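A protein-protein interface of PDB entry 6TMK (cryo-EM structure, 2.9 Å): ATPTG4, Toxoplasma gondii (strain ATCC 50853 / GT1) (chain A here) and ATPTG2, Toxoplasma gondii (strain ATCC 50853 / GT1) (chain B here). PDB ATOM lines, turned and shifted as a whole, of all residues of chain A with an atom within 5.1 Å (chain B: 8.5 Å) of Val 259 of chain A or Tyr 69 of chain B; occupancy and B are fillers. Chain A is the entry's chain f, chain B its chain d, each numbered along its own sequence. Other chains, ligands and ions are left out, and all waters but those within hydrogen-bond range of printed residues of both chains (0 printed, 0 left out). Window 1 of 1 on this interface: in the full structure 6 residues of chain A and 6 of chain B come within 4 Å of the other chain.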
ATOM      1  N   ILE A 252      30.061   5.905   1.837  1.00  0.00           N
ATOM      2  CA  ILE A 252      29.751   4.550   2.265  1.00  0.00           C
ATOM      3  C   ILE A 252      30.420   3.513   1.370  1.00  0.00           C
ATOM      4  O   ILE A 252      30.798   2.440   1.849  1.00  0.00           O
ATOM      5  CB  ILE A 252      28.232   4.344   2.324  1.00  0.00           C
ATOM      6  CG1 ILE A 252      27.663   5.076   3.533  1.00  0.00           C
ATOM      7  CG2 ILE A 252      27.898   2.879   2.391  1.00  0.00           C
ATOM      8  CD1 ILE A 252      26.198   5.310   3.470  1.00  0.00           C
ATOM      9  N   ASN A 256      32.505   1.610   4.511  1.00  0.00           N
ATOM     10  CA  ASN A 256      31.155   1.165   4.826  1.00  0.00           C
ATOM     11  C   ASN A 256      30.747   1.487   6.253  1.00  0.00           C
ATOM     12  O   ASN A 256      29.561   1.380   6.575  1.00  0.00           O
ATOM     13  CB  ASN A 256      31.013  -0.341   4.610  1.00  0.00           C
ATOM     14  CG  ASN A 256      31.269  -0.762   3.185  1.00  0.00           C
ATOM     15  OD1 ASN A 256      32.088  -1.634   2.925  1.00  0.00           O
ATOM     16  ND2 ASN A 256      30.555  -0.162   2.257  1.00  0.00           N
ATOM     17  N   LEU A 257      31.685   1.874   7.113  1.00  0.00           N
ATOM     18  CA  LEU A 257      31.357   2.137   8.506  1.00  0.00           C
ATOM     19  C   LEU A 257      30.565   3.417   8.697  1.00  0.00           C
ATOM     20  O   LEU A 257      30.151   3.700   9.825  1.00  0.00           O
ATOM     21  CB  LEU A 257      32.633   2.194   9.340  1.00  0.00           C
ATOM     22  CG  LEU A 257      33.524   0.956   9.281  1.00  0.00           C
ATOM     23  CD1 LEU A 257      34.777   1.161  10.095  1.00  0.00           C
ATOM     24  CD2 LEU A 257      32.782  -0.265   9.759  1.00  0.00           C
ATOM     25  N   ASN A 258      30.341   4.195   7.641  1.00  0.00           N
ATOM     26  CA  ASN A 258      29.515   5.386   7.752  1.00  0.00           C
ATOM     27  C   ASN A 258      28.031   5.063   7.853  1.00  0.00           C
ATOM     28  O   ASN A 258      27.238   5.961   8.156  1.00  0.00           O
ATOM     29  CB  ASN A 258      29.762   6.305   6.561  1.00  0.00           C
ATOM     30  CG  ASN A 258      31.141   6.920   6.577  1.00  0.00           C
ATOM     31  OD1 ASN A 258      31.404   7.860   7.321  1.00  0.00           O
ATOM     32  ND2 ASN A 258      32.030   6.390   5.759  1.00  0.00           N
ATOM     33  N   VAL A 259      27.634   3.813   7.607  1.00  0.00           N
ATOM     34  CA  VAL A 259      26.243   3.433   7.811  1.00  0.00           C
ATOM     35  C   VAL A 259      25.867   3.579   9.275  1.00  0.00           C
ATOM     36  O   VAL A 259      24.731   3.939   9.600  1.00  0.00           O
ATOM     37  CB  VAL A 259      26.000   1.995   7.315  1.00  0.00           C
ATOM     38  CG1 VAL A 259      26.360   1.868   5.866  1.00  0.00           C
ATOM     39  CG2 VAL A 259      26.794   1.009   8.134  1.00  0.00           C
ATOM     40  N   TYR A 260      26.807   3.308  10.180  1.00  0.00           N
ATOM     41  CA  TYR A 260      26.543   3.515  11.597  1.00  0.00           C
ATOM     42  C   TYR A 260      26.320   4.987  11.900  1.00  0.00           C
ATOM     43  O   TYR A 260      25.387   5.348  12.627  1.00  0.00           O
ATOM     44  CB  TYR A 260      27.702   2.979  12.427  1.00  0.00           C
ATOM     45  CG  TYR A 260      27.867   1.487  12.374  1.00  0.00           C
ATOM     46  CD1 TYR A 260      27.046   0.654  13.109  1.00  0.00           C
ATOM     47  CD2 TYR A 260      28.853   0.910  11.599  1.00  0.00           C
ATOM     48  CE1 TYR A 260      27.197  -0.710  13.063  1.00  0.00           C
ATOM     49  CE2 TYR A 260      29.010  -0.450  11.550  1.00  0.00           C
ATOM     50  CZ  TYR A 260      28.183  -1.255  12.283  1.00  0.00           C
ATOM     51  OH  TYR A 260      28.343  -2.615  12.231  1.00  0.00           O
ATOM     52  N   ARG A 261      27.167   5.853  11.346  1.00  0.00           N
ATOM     53  CA  ARG A 261      26.978   7.287  11.509  1.00  0.00           C
ATOM     54  C   ARG A 261      25.608   7.722  11.014  1.00  0.00           C
ATOM     55  O   ARG A 261      24.916   8.502  11.676  1.00  0.00           O
ATOM     56  CB  ARG A 261      28.072   8.038  10.756  1.00  0.00           C
ATOM     57  CG  ARG A 261      28.094   9.515  11.004  1.00  0.00           C
ATOM     58  CD  ARG A 261      29.146  10.188  10.157  1.00  0.00           C
ATOM     59  NE  ARG A 261      28.746  10.279   8.758  1.00  0.00           N
ATOM     60  CZ  ARG A 261      29.579  10.530   7.757  1.00  0.00           C
ATOM     61  NH1 ARG A 261      30.872  10.712   7.987  1.00  0.00           N
ATOM     62  NH2 ARG A 261      29.115  10.598   6.522  1.00  0.00           N
ATOM     63  N   LYS A 262      25.202   7.227   9.846  1.00  0.00           N
ATOM     64  CA  LYS A 262      23.892   7.556   9.305  1.00  0.00           C
ATOM     65  C   LYS A 262      22.755   6.862  10.035  1.00  0.00           C
ATOM     66  O   LYS A 262      21.592   7.201   9.798  1.00  0.00           O
ATOM     67  CB  LYS A 262      23.840   7.202   7.825  1.00  0.00           C
ATOM     68  CG  LYS A 262      24.823   7.958   6.970  1.00  0.00           C
ATOM     69  CD  LYS A 262      24.659   9.458   7.085  1.00  0.00           C
ATOM     70  CE  LYS A 262      23.271   9.906   6.689  1.00  0.00           C
ATOM     71  NZ  LYS A 262      23.182  11.388   6.593  1.00  0.00           N
ATOM     72  N   GLY A 263      23.057   5.906  10.905  1.00  0.00           N
ATOM     73  CA  GLY A 263      22.036   5.237  11.674  1.00  0.00           C
ATOM     74  C   GLY A 263      21.306   4.141  10.944  1.00  0.00           C
ATOM     75  O   GLY A 263      20.269   3.679  11.432  1.00  0.00           O
ATOM     76  N   TRP A 264      21.805   3.707   9.798  1.00  0.00           N
ATOM     77  CA  TRP A 264      21.135   2.655   9.069  1.00  0.00           C
ATOM     78  C   TRP A 264      21.353   1.322   9.778  1.00  0.00           C
ATOM     79  O   TRP A 264      22.354   1.137  10.473  1.00  0.00           O
ATOM     80  CB  TRP A 264      21.664   2.573   7.644  1.00  0.00           C
ATOM     81  CG  TRP A 264      21.371   3.769   6.822  1.00  0.00           C
ATOM     82  CD1 TRP A 264      20.688   4.874   7.201  1.00  0.00           C
ATOM     83  CD2 TRP A 264      21.755   3.981   5.465  1.00  0.00           C
ATOM     84  NE1 TRP A 264      20.620   5.769   6.170  1.00  0.00           N
ATOM     85  CE2 TRP A 264      21.270   5.241   5.089  1.00  0.00           C
ATOM     86  CE3 TRP A 264      22.462   3.227   4.531  1.00  0.00           C
ATOM     87  CZ2 TRP A 264      21.466   5.762   3.824  1.00  0.00           C
ATOM     88  CZ3 TRP A 264      22.654   3.747   3.281  1.00  0.00           C
ATOM     89  CH2 TRP A 264      22.160   4.998   2.935  1.00  0.00           C
ATOM     90  N   PRO A 265      20.435   0.375   9.620  1.00  0.00           N
ATOM     91  CA  PRO A 265      20.632  -0.940  10.227  1.00  0.00           C
ATOM     92  C   PRO A 265      21.788  -1.678   9.573  1.00  0.00           C
ATOM     93  O   PRO A 265      22.295  -1.300   8.517  1.00  0.00           O
ATOM     94  CB  PRO A 265      19.297  -1.645   9.996  1.00  0.00           C
ATOM     95  CG  PRO A 265      18.697  -0.964   8.841  1.00  0.00           C
ATOM     96  CD  PRO A 265      19.169   0.452   8.878  1.00  0.00           C
ATOM     97  N   VAL A 266      22.219  -2.743  10.239  1.00  0.00           N
ATOM     98  CA  VAL A 266      23.244  -3.624   9.700  1.00  0.00           C
ATOM     99  C   VAL A 266      22.808  -5.070   9.873  1.00  0.00           C
ATOM    100  O   VAL A 266      23.570  -5.999   9.587  1.00  0.00           O
ATOM    101  CB  VAL A 266      24.599  -3.375  10.380  1.00  0.00           C
ATOM    102  CG1 VAL A 266      25.205  -2.092   9.872  1.00  0.00           C
ATOM    103  CG2 VAL A 266      24.434  -3.331  11.882  1.00  0.00           C
ATOM    104  N   GLU B  65      30.472  -3.727  -7.978  1.00  0.00           N
ATOM    105  CA  GLU B  65      30.261  -2.902  -6.806  1.00  0.00           C
ATOM    106  C   GLU B  65      29.685  -3.726  -5.659  1.00  0.00           C
ATOM    107  O   GLU B  65      29.368  -4.910  -5.793  1.00  0.00           O
ATOM    108  CB  GLU B  65      29.350  -1.720  -7.133  1.00  0.00           C
ATOM    109  CG  GLU B  65      27.939  -2.067  -7.570  1.00  0.00           C
ATOM    110  CD  GLU B  65      27.832  -2.275  -9.066  1.00  0.00           C
ATOM    111  OE1 GLU B  65      28.870  -2.520  -9.714  1.00  0.00           O
ATOM    112  OE2 GLU B  65      26.709  -2.175  -9.600  1.00  0.00           O
ATOM    113  N   HIS B  66      29.562  -3.068  -4.513  1.00  0.00           N
ATOM    114  CA  HIS B  66      28.898  -3.656  -3.362  1.00  0.00           C
ATOM    115  C   HIS B  66      27.503  -4.143  -3.719  1.00  0.00           C
ATOM    116  O   HIS B  66      26.788  -3.516  -4.502  1.00  0.00           O
ATOM    117  CB  HIS B  66      28.810  -2.614  -2.254  1.00  0.00           C
ATOM    118  CG  HIS B  66      28.894  -3.175  -0.874  1.00  0.00           C
ATOM    119  ND1 HIS B  66      27.795  -3.660  -0.201  1.00  0.00           N
ATOM    120  CD2 HIS B  66      29.940  -3.305  -0.029  1.00  0.00           C
ATOM    121  CE1 HIS B  66      28.165  -4.076   0.994  1.00  0.00           C
ATOM    122  NE2 HIS B  66      29.462  -3.873   1.124  1.00  0.00           N
ATOM    123  N   ALA B  67      27.115  -5.268  -3.123  1.00  0.00           N
ATOM    124  CA  ALA B  67      25.841  -5.878  -3.466  1.00  0.00           C
ATOM    125  C   ALA B  67      24.675  -5.126  -2.841  1.00  0.00           C
ATOM    126  O   ALA B  67      23.610  -5.005  -3.455  1.00  0.00           O
ATOM    127  CB  ALA B  67      25.831  -7.337  -3.020  1.00  0.00           C
ATOM    128  N   THR B  68      24.854  -4.614  -1.625  1.00  0.00           N
ATOM    129  CA  THR B  68      23.765  -4.016  -0.871  1.00  0.00           C
ATOM    130  C   THR B  68      23.866  -2.505  -0.737  1.00  0.00           C
ATOM    131  O   THR B  68      22.836  -1.846  -0.596  1.00  0.00           O
ATOM    132  CB  THR B  68      23.683  -4.644   0.525  1.00  0.00           C
ATOM    133  OG1 THR B  68      22.701  -3.964   1.314  1.00  0.00           O
ATOM    134  CG2 THR B  68      24.995  -4.586   1.215  1.00  0.00           C
ATOM    135  N   TYR B  69      25.069  -1.943  -0.770  1.00  0.00           N
ATOM    136  CA  TYR B  69      25.268  -0.497  -0.766  1.00  0.00           C
ATOM    137  C   TYR B  69      25.894  -0.128  -2.103  1.00  0.00           C
ATOM    138  O   TYR B  69      27.102   0.070  -2.215  1.00  0.00           O
ATOM    139  CB  TYR B  69      26.133  -0.049   0.391  1.00  0.00           C
ATOM    140  CG  TYR B  69      25.611  -0.460   1.735  1.00  0.00           C
ATOM    141  CD1 TYR B  69      24.350  -0.087   2.150  1.00  0.00           C
ATOM    142  CD2 TYR B  69      26.381  -1.219   2.592  1.00  0.00           C
ATOM    143  CE1 TYR B  69      23.869  -0.464   3.370  1.00  0.00           C
ATOM    144  CE2 TYR B  69      25.907  -1.599   3.815  1.00  0.00           C
ATOM    145  CZ  TYR B  69      24.650  -1.219   4.201  1.00  0.00           C
ATOM    146  OH  TYR B  69      24.171  -1.600   5.428  1.00  0.00           O
ATOM    147  N   ASN B  70      25.053  -0.005  -3.115  1.00  0.00           N
ATOM    148  CA  ASN B  70      25.508   0.243  -4.468  1.00  0.00           C
ATOM    149  C   ASN B  70      25.155   1.660  -4.905  1.00  0.00           C
ATOM    150  O   ASN B  70      24.457   2.418  -4.217  1.00  0.00           O
ATOM    151  CB  ASN B  70      24.934  -0.801  -5.424  1.00  0.00           C
ATOM    152  CG  ASN B  70      23.431  -0.812  -5.449  1.00  0.00           C
ATOM    153  OD1 ASN B  70      22.792   0.144  -5.881  1.00  0.00           O
ATOM    154  ND2 ASN B  70      22.853  -1.903  -4.993  1.00  0.00           N
ATOM    155  N   TYR B  71      25.634   1.989  -6.103  1.00  0.00           N
ATOM    156  CA  TYR B  71      25.591   3.361  -6.580  1.00  0.00           C
ATOM    157  C   TYR B  71      24.156   3.828  -6.745  1.00  0.00           C
ATOM    158  O   TYR B  71      23.783   4.911  -6.281  1.00  0.00           O
ATOM    159  CB  TYR B  71      26.340   3.465  -7.905  1.00  0.00           C
ATOM    160  CG  TYR B  71      27.687   2.791  -7.922  1.00  0.00           C
ATOM    161  CD1 TYR B  71      28.627   3.037  -6.940  1.00  0.00           C
ATOM    162  CD2 TYR B  71      28.015   1.901  -8.926  1.00  0.00           C
ATOM    163  CE1 TYR B  71      29.852   2.416  -6.963  1.00  0.00           C
ATOM    164  CE2 TYR B  71      29.233   1.281  -8.954  1.00  0.00           C
ATOM    165  CZ  TYR B  71      30.148   1.539  -7.975  1.00  0.00           C
ATOM    166  OH  TYR B  71      31.363   0.907  -8.018  1.00  0.00           O
ATOM    167  N   PHE B  72      23.328   3.010  -7.389  1.00  0.00           N
ATOM    168  CA  PHE B  72      21.968   3.430  -7.668  1.00  0.00           C
ATOM    169  C   PHE B  72      21.152   3.565  -6.396  1.00  0.00           C
ATOM    170  O   PHE B  72      20.342   4.486  -6.271  1.00  0.00           O
ATOM    171  CB  PHE B  72      21.274   2.457  -8.606  1.00  0.00           C
ATOM    172  CG  PHE B  72      19.841   2.790  -8.818  1.00  0.00           C
ATOM    173  CD1 PHE B  72      19.485   3.821  -9.656  1.00  0.00           C
ATOM    174  CD2 PHE B  72      18.853   2.116  -8.138  1.00  0.00           C
ATOM    175  CE1 PHE B  72      18.177   4.149  -9.835  1.00  0.00           C
ATOM    176  CE2 PHE B  72      17.545   2.442  -8.316  1.00  0.00           C
ATOM    177  CZ  PHE B  72      17.205   3.464  -9.166  1.00  0.00           C
ATOM    178  N   VAL B  73      21.308   2.633  -5.461  1.00  0.00           N
ATOM    179  CA  VAL B  73      20.467   2.678  -4.278  1.00  0.00           C
ATOM    180  C   VAL B  73      20.860   3.862  -3.407  1.00  0.00           C
ATOM    181  O   VAL B  73      19.996   4.561  -2.866  1.00  0.00           O
ATOM    182  CB  VAL B  73      20.533   1.342  -3.514  1.00  0.00           C
ATOM    183  CG1 VAL B  73      21.810   1.215  -2.740  1.00  0.00           C
ATOM    184  CG2 VAL B  73      19.334   1.171  -2.628  1.00  0.00           C
ATOM    185  N   LEU B  74      22.161   4.154  -3.311  1.00  0.00           N
ATOM    186  CA  LEU B  74      22.570   5.366  -2.610  1.00  0.00           C
ATOM    187  C   LEU B  74      22.049   6.617  -3.313  1.00  0.00           C
ATOM    188  O   LEU B  74      21.574   7.557  -2.662  1.00  0.00           O
ATOM    189  CB  LEU B  74      24.089   5.405  -2.494  1.00  0.00           C
ATOM    190  CG  LEU B  74      24.737   4.299  -1.665  1.00  0.00           C
ATOM    191  CD1 LEU B  74      26.231   4.368  -1.755  1.00  0.00           C
ATOM    192  CD2 LEU B  74      24.312   4.359  -0.227  1.00  0.00           C
ATOM    193  N   PHE B  75      22.100   6.633  -4.643  1.00  0.00           N
ATOM    194  CA  PHE B  75      21.624   7.779  -5.406  1.00  0.00           C
ATOM    195  C   PHE B  75      20.138   8.027  -5.171  1.00  0.00           C
ATOM    196  O   PHE B  75      19.718   9.156  -4.888  1.00  0.00           O
ATOM    197  CB  PHE B  75      21.922   7.557  -6.887  1.00  0.00           C
ATOM    198  CG  PHE B  75      21.402   8.632  -7.780  1.00  0.00           C
ATOM    199  CD1 PHE B  75      21.996   9.872  -7.808  1.00  0.00           C
ATOM    200  CD2 PHE B  75      20.324   8.396  -8.604  1.00  0.00           C
ATOM    201  CE1 PHE B  75      21.519  10.857  -8.626  1.00  0.00           C
ATOM    202  CE2 PHE B  75      19.844   9.379  -9.423  1.00  0.00           C
ATOM    203  CZ  PHE B  75      20.443  10.611  -9.436  1.00  0.00           C
ATOM    204  N   ARG B  77      18.256   6.936  -2.762  1.00  0.00           N
ATOM    205  CA  ARG B  77      18.031   7.328  -1.380  1.00  0.00           C
ATOM    206  C   ARG B  77      18.363   8.794  -1.155  1.00  0.00           C
ATOM    207  O   ARG B  77      17.744   9.446  -0.308  1.00  0.00           O
ATOM    208  CB  ARG B  77      18.835   6.433  -0.451  1.00  0.00           C
ATOM    209  CG  ARG B  77      18.248   5.058  -0.334  1.00  0.00           C
ATOM    210  CD  ARG B  77      19.087   4.121   0.470  1.00  0.00           C
ATOM    211  NE  ARG B  77      18.629   2.751   0.319  1.00  0.00           N
ATOM    212  CZ  ARG B  77      19.186   1.702   0.908  1.00  0.00           C
ATOM    213  NH1 ARG B  77      20.219   1.857   1.704  1.00  0.00           N
ATOM    214  NH2 ARG B  77      18.692   0.497   0.709  1.00  0.00           N
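A ring nitrogen (ND1) of His 66 of chain B lies close to the backbone NH (N) of Thr 68 of chain B, 3.4 Å away. The backbone carbonyl oxygen (O) of Val 259 of chain A sits at hydrogen-bond distance from the backbone NH (N) of Trp 264 of chain A, at 2.9 Å. O of Ile 252 of chain A lies within hydrogen-bond range of ND2 of Asn 256 of chain A (2.6 Å). A ring nitrogen (ND1) of His 66 of chain B sits at hydrogen-bond distance from the backbone NH (N) of Tyr 69 of chain B.
Among the printed residues, pairs that only touch across the chains: Trp 264 of chain A with Arg 77 of chain B (3.5 Å), Pro 265 of chain A with Tyr 69 of chain B (3.6 Å), Trp 264 of chain A with Leu 74 of chain B (3.9 Å), Asn 256 of chain A with His 66 of chain B (3.9 Å), Val 259 of chain A with Tyr 69 of chain B (3.9 Å) and Ile 252 of chain A with Tyr 69 of chain B (3.96 Å).
Val 259 of chain A touches one residue of chain B. Of the printed residues of chain A, Leu 74 of chain B touches Trp 264. Of the printed residues of chain B, Pro 265 of chain A touches Tyr 69. Printed residues of chain A within 4 Å of Arg 77 of chain B: Trp 264. Of the printed residues of chain B, Ile 252 of chain A touches Tyr 69 (3.96 Å). Tyr 260 of chain A touches none of the printed residues of chain B. Phe 72 of chain B touches none of the printed residues of chain A. The nearest residue of chain B that does not touch Val 259 of chain A is Leu 74 of chain B (6.9 Å). The nearest residue of chain A that does not touch Tyr 69 of chain B is Trp 264 of chain A (4.1 Å). The nearest printed residue of chain B that does not touch Pro 265 of chain A is Arg 77 of chain B (7.4 Å).
Printed residues of chain A that touch a printed residue of chain B: Ile 252, Asn 256, Val 259, Trp 264 and Pro 265. Hydrophobic or aromatic side chains of chain A within 4 Å of the printed part of chain B: Ile 252, Val 259 and Trp 264. Of the 12 printed residues of chain B, 4 touch a printed residue of chain A. Among the printed residues, 6 pairs touch across the chains. Among the printed residues, no Asp or Glu carboxylate lies within 4 Å of a Lys or Arg side-chain nitrogen of the other chain.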
